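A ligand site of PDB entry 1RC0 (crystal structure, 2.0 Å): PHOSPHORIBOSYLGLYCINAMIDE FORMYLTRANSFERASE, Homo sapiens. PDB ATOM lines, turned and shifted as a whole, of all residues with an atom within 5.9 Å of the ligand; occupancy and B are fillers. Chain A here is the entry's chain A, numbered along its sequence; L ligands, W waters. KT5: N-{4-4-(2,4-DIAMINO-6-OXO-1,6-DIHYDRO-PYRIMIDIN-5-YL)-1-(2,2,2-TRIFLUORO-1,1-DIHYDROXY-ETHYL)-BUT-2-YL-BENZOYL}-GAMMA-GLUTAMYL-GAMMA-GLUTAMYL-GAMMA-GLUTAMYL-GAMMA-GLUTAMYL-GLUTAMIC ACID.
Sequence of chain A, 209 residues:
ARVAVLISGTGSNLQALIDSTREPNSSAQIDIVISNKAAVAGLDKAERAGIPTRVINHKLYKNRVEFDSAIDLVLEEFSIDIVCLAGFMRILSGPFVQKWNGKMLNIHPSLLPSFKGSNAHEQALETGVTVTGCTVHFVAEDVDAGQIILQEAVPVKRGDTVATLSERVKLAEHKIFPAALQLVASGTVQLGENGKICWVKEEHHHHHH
N of Gly 117 lies within hydrogen-bond range of OD2 of Asp 144 (2.9 Å). The guanidinium group (NH1) of Arg 64 sits at hydrogen-bond distance from the backbone carbonyl oxygen (O) of Ile 91 (2.8 Å). ND1 of His 108 sits close to OD2 of Asp 144 (3.2 Å). The backbone NH (N) of Asn 106 is in hydrogen-bond range of the backbone carbonyl oxygen (O) of His 137 (2.9 Å).
Water W4 lies within hydrogen-bond range of the backbone carbonyl oxygen of Phe 88 (2.7 Å), the backbone carbonyl oxygen of Arg 90 (2.7 Å) and a nitrogen (N8) of the ligand (2.8 Å). Water W1 bridges the backbone carbonyl oxygen (O) of Ile 107 (2.7 Å) and the backbone NH (N) of Gly 87 (3.1 Å). Water W5 lies within hydrogen-bond range of the backbone carbonyl oxygen (O) of Phe 88 (2.8 Å), the side-chain amide oxygen (OD1) of Asn 106 (2.8 Å) and the backbone NH (N) of Gly 87 (3.4 Å).
A nitrogen (N3) of the ligand lies close to the backbone carbonyl oxygen of Ala 140, 2.9 Å away. Residues that only touch the ligand: Leu 85 (3.7 Å), Phe 88 (3.98 Å), Val 97 (3.8 Å), Pro 109 (3.4 Å), Ser 118 (3.6 Å), His 137 (3.9 Å), Val 139 (3.7 Å), Asp 142 (3.9 Å) and Val 143 (3.5 Å). Within 4 Å of the ligand: Arg 64, Leu 85, Phe 88, Met 89, Arg 90, Ile 91, Leu 92, Val 97, Asn 106, His 108, Pro 109, Gly 117, Ser 118, His 137, Val 139, Ala 140, Glu 141, Asp 142, Val 143 and Asp 144. Along chain A the residues within 4 Å of the ligand span positions 64 to 144. The nearest printed residue that does not touch the ligand is Ile 107 (4.002 Å).
A nitrogen (N2) of the ligand sits at hydrogen-bond distance from the backbone carbonyl oxygen (O) of Leu 92, 3.0 Å away. The side-chain carboxylate of Asp 144 is in hydrogen-bond range of an oxygen (OA2) of the ligand, at 2.6 Å. The backbone carbonyl oxygen (O) of Arg 90 lies within hydrogen-bond range of a nitrogen (N8) of the ligand, at 2.9 Å. The backbone NH (N) of Asp 144 is in hydrogen-bond range of an oxygen (O1) of the ligand. O of Met 89 lies within hydrogen-bond range of N1A of the ligand (3.1 Å). An oxygen (O11) of the ligand lies within salt-bridge range of the guanidinium group of Arg 64. A nitrogen (N1) of the ligand lies within hydrogen-bond range of the backbone NH (N) of Leu 92 (3.0 Å). A ring nitrogen (ND1) of His 108 sits at hydrogen-bond distance from an oxygen (OA2) of the ligand. N of Ile 91 is in hydrogen-bond range of O1A of the ligand (3.1 Å). An oxygen (O11) of the ligand lies within salt-bridge range of the guanidinium group (NH1) of Arg 90 (3.4 Å). The backbone carbonyl oxygen of Glu 141 sits at hydrogen-bond distance from a nitrogen (N2) of the ligand, at 3.0 Å. OA2 of the ligand is in hydrogen-bond range of ND2 of Asn 106 (3.2 Å). An oxygen (OA1) of the ligand is in hydrogen-bond range of the backbone carbonyl oxygen of Gly 117.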
ATOM      1  N   ARG A  64      40.791  21.713 -38.391  1.00  0.00           N
ATOM      2  CA  ARG A  64      40.442  21.373 -37.019  1.00  0.00           C
ATOM      3  C   ARG A  64      41.567  20.654 -36.278  1.00  0.00           C
ATOM      4  O   ARG A  64      41.861  20.981 -35.128  1.00  0.00           O
ATOM      5  CB  ARG A  64      39.163  20.520 -36.999  1.00  0.00           C
ATOM      6  CG  ARG A  64      37.882  21.318 -36.936  1.00  0.00           C
ATOM      7  CD  ARG A  64      36.633  20.563 -37.396  1.00  0.00           C
ATOM      8  NE  ARG A  64      35.658  21.462 -38.032  1.00  0.00           N
ATOM      9  CZ  ARG A  64      34.955  22.395 -37.396  1.00  0.00           C
ATOM     10  NH1 ARG A  64      35.079  22.583 -36.087  1.00  0.00           N
ATOM     11  NH2 ARG A  64      34.094  23.151 -38.073  1.00  0.00           N
ATOM     12  N   LEU A  85      33.788  21.817 -21.380  1.00  0.00           N
ATOM     13  CA  LEU A  85      33.415  22.791 -22.399  1.00  0.00           C
ATOM     14  C   LEU A  85      32.283  23.660 -21.831  1.00  0.00           C
ATOM     15  O   LEU A  85      31.197  23.154 -21.530  1.00  0.00           O
ATOM     16  CB  LEU A  85      32.983  22.112 -23.711  1.00  0.00           C
ATOM     17  CG  LEU A  85      33.930  21.125 -24.423  1.00  0.00           C
ATOM     18  CD1 LEU A  85      33.369  20.722 -25.764  1.00  0.00           C
ATOM     19  CD2 LEU A  85      35.312  21.696 -24.610  1.00  0.00           C
ATOM     20  N   GLY A  87      30.375  26.701 -23.091  1.00  0.00           N
ATOM     21  CA  GLY A  87      30.119  27.559 -24.234  1.00  0.00           C
ATOM     22  C   GLY A  87      31.256  27.591 -25.262  1.00  0.00           C
ATOM     23  O   GLY A  87      31.376  28.555 -26.006  1.00  0.00           O
ATOM     24  N   PHE A  88      32.084  26.540 -25.291  1.00  0.00           N
ATOM     25  CA  PHE A  88      33.059  26.353 -26.374  1.00  0.00           C
ATOM     26  C   PHE A  88      32.290  26.026 -27.653  1.00  0.00           C
ATOM     27  O   PHE A  88      31.442  25.119 -27.646  1.00  0.00           O
ATOM     28  CB  PHE A  88      34.056  25.249 -26.030  1.00  0.00           C
ATOM     29  CG  PHE A  88      35.216  25.146 -26.997  1.00  0.00           C
ATOM     30  CD1 PHE A  88      36.220  26.121 -27.019  1.00  0.00           C
ATOM     31  CD2 PHE A  88      35.315  24.073 -27.878  1.00  0.00           C
ATOM     32  CE1 PHE A  88      37.297  26.027 -27.908  1.00  0.00           C
ATOM     33  CE2 PHE A  88      36.393  23.979 -28.767  1.00  0.00           C
ATOM     34  CZ  PHE A  88      37.380  24.956 -28.786  1.00  0.00           C
ATOM     35  N   MET A  89      32.590  26.747 -28.730  1.00  0.00           N
ATOM     36  CA  MET A  89      31.731  26.743 -29.920  1.00  0.00           C
ATOM     37  C   MET A  89      32.358  26.085 -31.144  1.00  0.00           C
ATOM     38  O   MET A  89      31.758  26.092 -32.219  1.00  0.00           O
ATOM     39  CB  MET A  89      31.294  28.168 -30.258  1.00  0.00           C
ATOM     40  CG  MET A  89      30.195  28.709 -29.351  1.00  0.00           C
ATOM     41  SD  MET A  89      28.738  27.652 -29.356  1.00  0.00           S
ATOM     42  CE  MET A  89      28.540  27.348 -27.612  1.00  0.00           C
ATOM     43  N   ARG A  90      33.545  25.513 -30.985  1.00  0.00           N
ATOM     44  CA  ARG A  90      34.192  24.792 -32.076  1.00  0.00           C
ATOM     45  C   ARG A  90      33.989  23.289 -31.946  1.00  0.00           C
ATOM     46  O   ARG A  90      34.231  22.713 -30.887  1.00  0.00           O
ATOM     47  CB  ARG A  90      35.690  25.115 -32.146  1.00  0.00           C
ATOM     48  CG  ARG A  90      36.014  26.596 -32.364  1.00  0.00           C
ATOM     49  CD  ARG A  90      35.324  27.217 -33.571  1.00  0.00           C
ATOM     50  NE  ARG A  90      35.884  26.719 -34.824  1.00  0.00           N
ATOM     51  CZ  ARG A  90      35.393  26.980 -36.028  1.00  0.00           C
ATOM     52  NH1 ARG A  90      34.313  27.739 -36.173  1.00  0.00           N
ATOM     53  NH2 ARG A  90      35.986  26.491 -37.108  1.00  0.00           N
ATOM     54  N   ILE A  91      33.543  22.651 -33.019  1.00  0.00           N
ATOM     55  CA  ILE A  91      33.474  21.198 -33.045  1.00  0.00           C
ATOM     56  C   ILE A  91      34.895  20.630 -33.074  1.00  0.00           C
ATOM     57  O   ILE A  91      35.747  21.099 -33.832  1.00  0.00           O
ATOM     58  CB  ILE A  91      32.613  20.697 -34.220  1.00  0.00           C
ATOM     59  CG1 ILE A  91      31.168  21.230 -34.085  1.00  0.00           C
ATOM     60  CG2 ILE A  91      32.606  19.180 -34.280  1.00  0.00           C
ATOM     61  CD1 ILE A  91      30.426  21.363 -35.403  1.00  0.00           C
ATOM     62  N   LEU A  92      35.136  19.645 -32.221  1.00  0.00           N
ATOM     63  CA  LEU A  92      36.461  19.047 -32.124  1.00  0.00           C
ATOM     64  C   LEU A  92      36.610  17.850 -33.052  1.00  0.00           C
ATOM     65  O   LEU A  92      35.631  17.165 -33.384  1.00  0.00           O
ATOM     66  CB  LEU A  92      36.766  18.658 -30.670  1.00  0.00           C
ATOM     67  CG  LEU A  92      36.880  19.843 -29.706  1.00  0.00           C
ATOM     68  CD1 LEU A  92      36.554  19.418 -28.277  1.00  0.00           C
ATOM     69  CD2 LEU A  92      38.268  20.481 -29.770  1.00  0.00           C
ATOM     70  N   SER A  93      37.848  17.619 -33.491  1.00  0.00           N
ATOM     71  CA  SER A  93      38.185  16.539 -34.429  1.00  0.00           C
ATOM     72  C   SER A  93      38.192  15.174 -33.747  1.00  0.00           C
ATOM     73  O   SER A  93      38.335  15.088 -32.528  1.00  0.00           O
ATOM     74  CB  SER A  93      39.555  16.814 -35.060  1.00  0.00           C
ATOM     75  OG  SER A  93      40.609  16.574 -34.130  1.00  0.00           O
ATOM     76  N   VAL A  97      39.006  14.134 -29.748  1.00  0.00           N
ATOM     77  CA  VAL A  97      37.874  13.549 -29.027  1.00  0.00           C
ATOM     78  C   VAL A  97      38.220  12.145 -28.514  1.00  0.00           C
ATOM     79  O   VAL A  97      37.870  11.781 -27.379  1.00  0.00           O
ATOM     80  CB  VAL A  97      36.570  13.537 -29.895  1.00  0.00           C
ATOM     81  CG1 VAL A  97      35.489  12.694 -29.239  1.00  0.00           C
ATOM     82  CG2 VAL A  97      36.058  14.953 -30.133  1.00  0.00           C
ATOM     83  N   ASN A 106      30.643  18.336 -21.676  1.00  0.00           N
ATOM     84  CA  ASN A 106      30.005  19.498 -22.277  1.00  0.00           C
ATOM     85  C   ASN A 106      28.667  19.787 -21.593  1.00  0.00           C
ATOM     86  O   ASN A 106      27.999  18.867 -21.125  1.00  0.00           O
ATOM     87  CB  ASN A 106      29.752  19.259 -23.767  1.00  0.00           C
ATOM     88  CG  ASN A 106      29.066  20.441 -24.437  1.00  0.00           C
ATOM     89  OD1 ASN A 106      29.612  21.543 -24.482  1.00  0.00           O
ATOM     90  ND2 ASN A 106      27.863  20.221 -24.949  1.00  0.00           N
ATOM     91  N   ILE A 107      28.286  21.066 -21.544  1.00  0.00           N
ATOM     92  CA  ILE A 107      26.948  21.462 -21.126  1.00  0.00           C
ATOM     93  C   ILE A 107      26.148  21.900 -22.359  1.00  0.00           C
ATOM     94  O   ILE A 107      26.615  22.692 -23.179  1.00  0.00           O
ATOM     95  CB  ILE A 107      26.983  22.577 -20.007  1.00  0.00           C
ATOM     96  CG1 ILE A 107      25.585  22.898 -19.485  1.00  0.00           C
ATOM     97  CG2 ILE A 107      27.618  23.869 -20.515  1.00  0.00           C
ATOM     98  CD1 ILE A 107      25.020  21.879 -18.475  1.00  0.00           C
ATOM     99  N   HIS A 108      24.951  21.343 -22.487  1.00  0.00           N
ATOM    100  CA  HIS A 108      24.086  21.650 -23.606  1.00  0.00           C
ATOM    101  C   HIS A 108      22.705  22.086 -23.082  1.00  0.00           C
ATOM    102  O   HIS A 108      22.136  21.412 -22.233  1.00  0.00           O
ATOM    103  CB  HIS A 108      23.960  20.425 -24.521  1.00  0.00           C
ATOM    104  CG  HIS A 108      23.015  20.621 -25.661  1.00  0.00           C
ATOM    105  ND1 HIS A 108      23.378  21.259 -26.833  1.00  0.00           N
ATOM    106  CD2 HIS A 108      21.708  20.313 -25.793  1.00  0.00           C
ATOM    107  CE1 HIS A 108      22.335  21.306 -27.639  1.00  0.00           C
ATOM    108  NE2 HIS A 108      21.305  20.738 -27.034  1.00  0.00           N
ATOM    109  N   PRO A 109      22.169  23.210 -23.569  1.00  0.00           N
ATOM    110  CA  PRO A 109      20.924  23.787 -23.030  1.00  0.00           C
ATOM    111  C   PRO A 109      19.625  23.190 -23.628  1.00  0.00           C
ATOM    112  O   PRO A 109      18.722  23.931 -24.076  1.00  0.00           O
ATOM    113  CB  PRO A 109      21.063  25.267 -23.387  1.00  0.00           C
ATOM    114  CG  PRO A 109      21.833  25.257 -24.706  1.00  0.00           C
ATOM    115  CD  PRO A 109      22.730  24.039 -24.664  1.00  0.00           C
ATOM    116  N   LYS A 116      19.365  18.985 -30.600  1.00  0.00           N
ATOM    117  CA  LYS A 116      20.788  18.986 -30.830  1.00  0.00           C
ATOM    118  C   LYS A 116      21.178  20.258 -31.603  1.00  0.00           C
ATOM    119  O   LYS A 116      20.390  20.777 -32.419  1.00  0.00           O
ATOM    120  CB  LYS A 116      21.180  17.735 -31.619  1.00  0.00           C
ATOM    121  CG  LYS A 116      21.048  16.446 -30.802  1.00  0.00           C
ATOM    122  CD  LYS A 116      21.059  15.209 -31.707  1.00  0.00           C
ATOM    123  CE  LYS A 116      20.914  13.915 -30.890  1.00  0.00           C
ATOM    124  NZ  LYS A 116      21.606  12.736 -31.525  1.00  0.00           N
ATOM    125  N   GLY A 117      22.385  20.774 -31.348  1.00  0.00           N
ATOM    126  CA  GLY A 117      22.868  21.929 -32.080  1.00  0.00           C
ATOM    127  C   GLY A 117      22.833  23.184 -31.242  1.00  0.00           C
ATOM    128  O   GLY A 117      22.305  23.200 -30.134  1.00  0.00           O
ATOM    129  N   SER A 118      23.380  24.265 -31.798  1.00  0.00           N
ATOM    130  CA  SER A 118      23.780  25.443 -31.020  1.00  0.00           C
ATOM    131  C   SER A 118      22.666  26.464 -30.772  1.00  0.00           C
ATOM    132  O   SER A 118      22.887  27.476 -30.081  1.00  0.00           O
ATOM    133  CB  SER A 118      24.951  26.144 -31.720  1.00  0.00           C
ATOM    134  OG  SER A 118      24.552  26.596 -33.014  1.00  0.00           O
ATOM    135  N   ASN A 119      21.484  26.217 -31.336  1.00  0.00           N
ATOM    136  CA  ASN A 119      20.329  27.096 -31.135  1.00  0.00           C
ATOM    137  C   ASN A 119      19.174  26.361 -30.450  1.00  0.00           C
ATOM    138  O   ASN A 119      18.038  26.412 -30.910  1.00  0.00           O
ATOM    139  CB  ASN A 119      19.854  27.628 -32.500  1.00  0.00           C
ATOM    140  CG  ASN A 119      19.481  26.498 -33.463  1.00  0.00           C
ATOM    141  OD1 ASN A 119      19.896  25.339 -33.290  1.00  0.00           O
ATOM    142  ND2 ASN A 119      18.685  26.823 -34.495  1.00  0.00           N
ATOM    143  N   HIS A 137      26.978  15.984 -20.727  1.00  0.00           N
ATOM    144  CA  HIS A 137      27.310  14.723 -21.372  1.00  0.00           C
ATOM    145  C   HIS A 137      28.802  14.663 -21.659  1.00  0.00           C
ATOM    146  O   HIS A 137      29.444  15.698 -21.852  1.00  0.00           O
ATOM    147  CB  HIS A 137      26.529  14.541 -22.694  1.00  0.00           C
ATOM    148  CG  HIS A 137      26.793  15.620 -23.702  1.00  0.00           C
ATOM    149  ND1 HIS A 137      27.624  15.439 -24.789  1.00  0.00           N
ATOM    150  CD2 HIS A 137      26.339  16.892 -23.796  1.00  0.00           C
ATOM    151  CE1 HIS A 137      27.676  16.547 -25.500  1.00  0.00           C
ATOM    152  NE2 HIS A 137      26.897  17.447 -24.924  1.00  0.00           N
ATOM    153  N   PHE A 138      29.342  13.443 -21.697  1.00  0.00           N
ATOM    154  CA  PHE A 138      30.671  13.237 -22.257  1.00  0.00           C
ATOM    155  C   PHE A 138      30.666  13.652 -23.719  1.00  0.00           C
ATOM    156  O   PHE A 138      29.678  13.463 -24.446  1.00  0.00           O
ATOM    157  CB  PHE A 138      31.069  11.768 -22.128  1.00  0.00           C
ATOM    158  CG  PHE A 138      31.500  11.379 -20.755  1.00  0.00           C
ATOM    159  CD1 PHE A 138      32.667  11.908 -20.198  1.00  0.00           C
ATOM    160  CD2 PHE A 138      30.732  10.514 -19.983  1.00  0.00           C
ATOM    161  CE1 PHE A 138      33.070  11.566 -18.903  1.00  0.00           C
ATOM    162  CE2 PHE A 138      31.128  10.153 -18.709  1.00  0.00           C
ATOM    163  CZ  PHE A 138      32.304  10.680 -18.162  1.00  0.00           C
ATOM    164  N   VAL A 139      31.772  14.235 -24.171  1.00  0.00           N
ATOM    165  CA  VAL A 139      31.917  14.611 -25.573  1.00  0.00           C
ATOM    166  C   VAL A 139      32.277  13.363 -26.401  1.00  0.00           C
ATOM    167  O   VAL A 139      33.249  12.664 -26.109  1.00  0.00           O
ATOM    168  CB  VAL A 139      32.963  15.750 -25.731  1.00  0.00           C
ATOM    169  CG1 VAL A 139      33.238  16.050 -27.198  1.00  0.00           C
ATOM    170  CG2 VAL A 139      32.473  17.012 -25.014  1.00  0.00           C
ATOM    171  N   ALA A 140      31.458  13.071 -27.414  1.00  0.00           N
ATOM    172  CA  ALA A 140      31.779  12.060 -28.415  1.00  0.00           C
ATOM    173  C   ALA A 140      31.928  12.710 -29.785  1.00  0.00           C
ATOM    174  O   ALA A 140      31.567  13.884 -29.961  1.00  0.00           O
ATOM    175  CB  ALA A 140      30.687  10.974 -28.451  1.00  0.00           C
ATOM    176  N   GLU A 141      32.430  11.962 -30.755  1.00  0.00           N
ATOM    177  CA  GLU A 141      32.660  12.471 -32.099  1.00  0.00           C
ATOM    178  C   GLU A 141      31.400  13.127 -32.680  1.00  0.00           C
ATOM    179  O   GLU A 141      31.458  14.265 -33.159  1.00  0.00           O
ATOM    180  CB  GLU A 141      33.145  11.359 -33.019  1.00  0.00           C
ATOM    181  CG  GLU A 141      34.180  11.825 -34.029  1.00  0.00           C
ATOM    182  CD  GLU A 141      34.753  10.671 -34.818  1.00  0.00           C
ATOM    183  OE1 GLU A 141      35.802  10.120 -34.399  1.00  0.00           O
ATOM    184  OE2 GLU A 141      34.162  10.308 -35.856  1.00  0.00           O
ATOM    185  N   ASP A 142      30.287  12.400 -32.633  1.00  0.00           N
ATOM    186  CA  ASP A 142      28.993  12.938 -33.016  1.00  0.00           C
ATOM    187  C   ASP A 142      28.558  14.027 -32.044  1.00  0.00           C
ATOM    188  O   ASP A 142      28.502  13.815 -30.832  1.00  0.00           O
ATOM    189  CB  ASP A 142      27.951  11.813 -33.044  1.00  0.00           C
ATOM    190  CG  ASP A 142      28.082  10.930 -34.264  1.00  0.00           C
ATOM    191  OD1 ASP A 142      29.189  10.848 -34.856  1.00  0.00           O
ATOM    192  OD2 ASP A 142      27.124  10.252 -34.696  1.00  0.00           O
ATOM    193  N   VAL A 143      28.223  15.173 -32.609  1.00  0.00           N
ATOM    194  CA  VAL A 143      27.916  16.378 -31.867  1.00  0.00           C
ATOM    195  C   VAL A 143      26.651  16.191 -31.029  1.00  0.00           C
ATOM    196  O   VAL A 143      25.622  15.716 -31.534  1.00  0.00           O
ATOM    197  CB  VAL A 143      27.749  17.559 -32.865  1.00  0.00           C
ATOM    198  CG1 VAL A 143      27.144  18.770 -32.210  1.00  0.00           C
ATOM    199  CG2 VAL A 143      29.091  17.896 -33.530  1.00  0.00           C
ATOM    200  N   ASP A 144      26.746  16.557 -29.748  1.00  0.00           N
ATOM    201  CA  ASP A 144      25.619  16.488 -28.789  1.00  0.00           C
ATOM    202  C   ASP A 144      25.010  15.100 -28.680  1.00  0.00           C
ATOM    203  O   ASP A 144      23.809  14.959 -28.461  1.00  0.00           O
ATOM    204  CB  ASP A 144      24.535  17.527 -29.135  1.00  0.00           C
ATOM    205  CG  ASP A 144      24.969  18.945 -28.884  1.00  0.00           C
ATOM    206  OD1 ASP A 144      25.829  19.171 -28.001  1.00  0.00           O
ATOM    207  OD2 ASP A 144      24.489  19.920 -29.512  1.00  0.00           O
ATOM    208  N   ALA A 145      25.852  14.073 -28.802  1.00  0.00           N
ATOM    209  CA  ALA A 145      25.377  12.685 -28.845  1.00  0.00           C
ATOM    210  C   ALA A 145      26.096  11.776 -27.842  1.00  0.00           C
ATOM    211  O   ALA A 145      25.774  10.594 -27.756  1.00  0.00           O
ATOM    212  CB  ALA A 145      25.544  12.131 -30.253  1.00  0.00           C
ATOM    213  N   GLY A 146      27.028  12.335 -27.068  1.00  0.00           N
ATOM    214  CA  GLY A 146      27.791  11.580 -26.099  1.00  0.00           C
ATOM    215  C   GLY A 146      26.988  11.115 -24.898  1.00  0.00           C
ATOM    216  O   GLY A 146      25.817  11.476 -24.756  1.00  0.00           O
HETATM  217  N2A KT5 L   1      28.376  30.131 -35.525  1.00  0.00           N
HETATM  218  CD1 KT5 L   1      29.364  29.458 -34.982  1.00  0.00           C
HETATM  219  OEB KT5 L   1      30.231  29.922 -34.248  1.00  0.00           O
HETATM  220  CG1 KT5 L   1      29.280  28.029 -35.370  1.00  0.00           C
HETATM  221  CB1 KT5 L   1      30.569  27.208 -35.213  1.00  0.00           C
HETATM  222  CA1 KT5 L   1      30.474  25.804 -35.697  1.00  0.00           C
HETATM  223  C1A KT5 L   1      31.827  25.163 -36.247  1.00  0.00           C
HETATM  224  O11 KT5 L   1      32.177  25.411 -37.387  1.00  0.00           O
HETATM  225  O1A KT5 L   1      32.580  24.334 -35.441  1.00  0.00           O
HETATM  226  N1A KT5 L   1      30.017  25.000 -34.495  1.00  0.00           N
HETATM  227  C   KT5 L   1      28.743  24.496 -34.316  1.00  0.00           C
HETATM  228  O   KT5 L   1      27.907  24.521 -35.201  1.00  0.00           O
HETATM  229  C14 KT5 L   1      28.428  23.969 -32.995  1.00  0.00           C
HETATM  230  C15 KT5 L   1      29.127  24.447 -31.755  1.00  0.00           C
HETATM  231  C16 KT5 L   1      28.860  23.835 -30.513  1.00  0.00           C
HETATM  232  C13 KT5 L   1      27.412  22.868 -32.919  1.00  0.00           C
HETATM  233  C12 KT5 L   1      27.117  22.234 -31.657  1.00  0.00           C
HETATM  234  C11 KT5 L   1      27.875  22.751 -30.413  1.00  0.00           C
HETATM  235  C10 KT5 L   1      27.757  22.147 -28.901  1.00  0.00           C
HETATM  236  C5  KT5 L   1      26.519  22.467 -27.940  1.00  0.00           C
HETATM  237  C6  KT5 L   1      26.436  23.968 -27.567  1.00  0.00           C
HETATM  238  F2  KT5 L   1      26.406  24.891 -28.592  1.00  0.00           F
HETATM  239  F1  KT5 L   1      27.638  24.123 -27.017  1.00  0.00           F
HETATM  240  F3  KT5 L   1      25.429  24.197 -26.692  1.00  0.00           F
HETATM  241  OA2 KT5 L   1      26.106  21.663 -27.195  1.00  0.00           O
HETATM  242  OA1 KT5 L   1      25.340  22.511 -29.014  1.00  0.00           O
HETATM  243  C1  KT5 L   1      28.119  20.657 -28.896  1.00  0.00           C
HETATM  244  C2  KT5 L   1      29.790  20.718 -28.626  1.00  0.00           C
HETATM  245  C3  KT5 L   1      30.359  19.481 -27.851  1.00  0.00           C
HETATM  246  C4  KT5 L   1      31.240  18.895 -28.914  1.00  0.00           C
HETATM  247  C7  KT5 L   1      32.492  19.206 -29.643  1.00  0.00           C
HETATM  248  N8  KT5 L   1      33.130  20.408 -29.467  1.00  0.00           N
HETATM  249  C9  KT5 L   1      30.743  17.696 -29.294  1.00  0.00           C
HETATM  250  O1  KT5 L   1      29.697  16.885 -28.831  1.00  0.00           O
HETATM  251  N3  KT5 L   1      31.384  16.705 -30.400  1.00  0.00           N
HETATM  252  C8  KT5 L   1      32.543  17.147 -30.989  1.00  0.00           C
HETATM  253  N2  KT5 L   1      33.126  16.460 -31.980  1.00  0.00           N
HETATM  254  N1  KT5 L   1      33.053  18.299 -30.621  1.00  0.00           N
HETATM  255  O   HOH W   1      28.124  24.824 -23.943  1.00  0.00           O
HETATM  256  O   HOH W   2      29.054  14.407 -28.244  1.00  0.00           O
HETATM  257  O   HOH W   3      24.010  27.018 -27.053  1.00  0.00           O
HETATM  258  O   HOH W   4      32.118  23.030 -29.167  1.00  0.00           O
HETATM  259  O   HOH W   5      30.417  24.065 -25.315  1.00  0.00           O
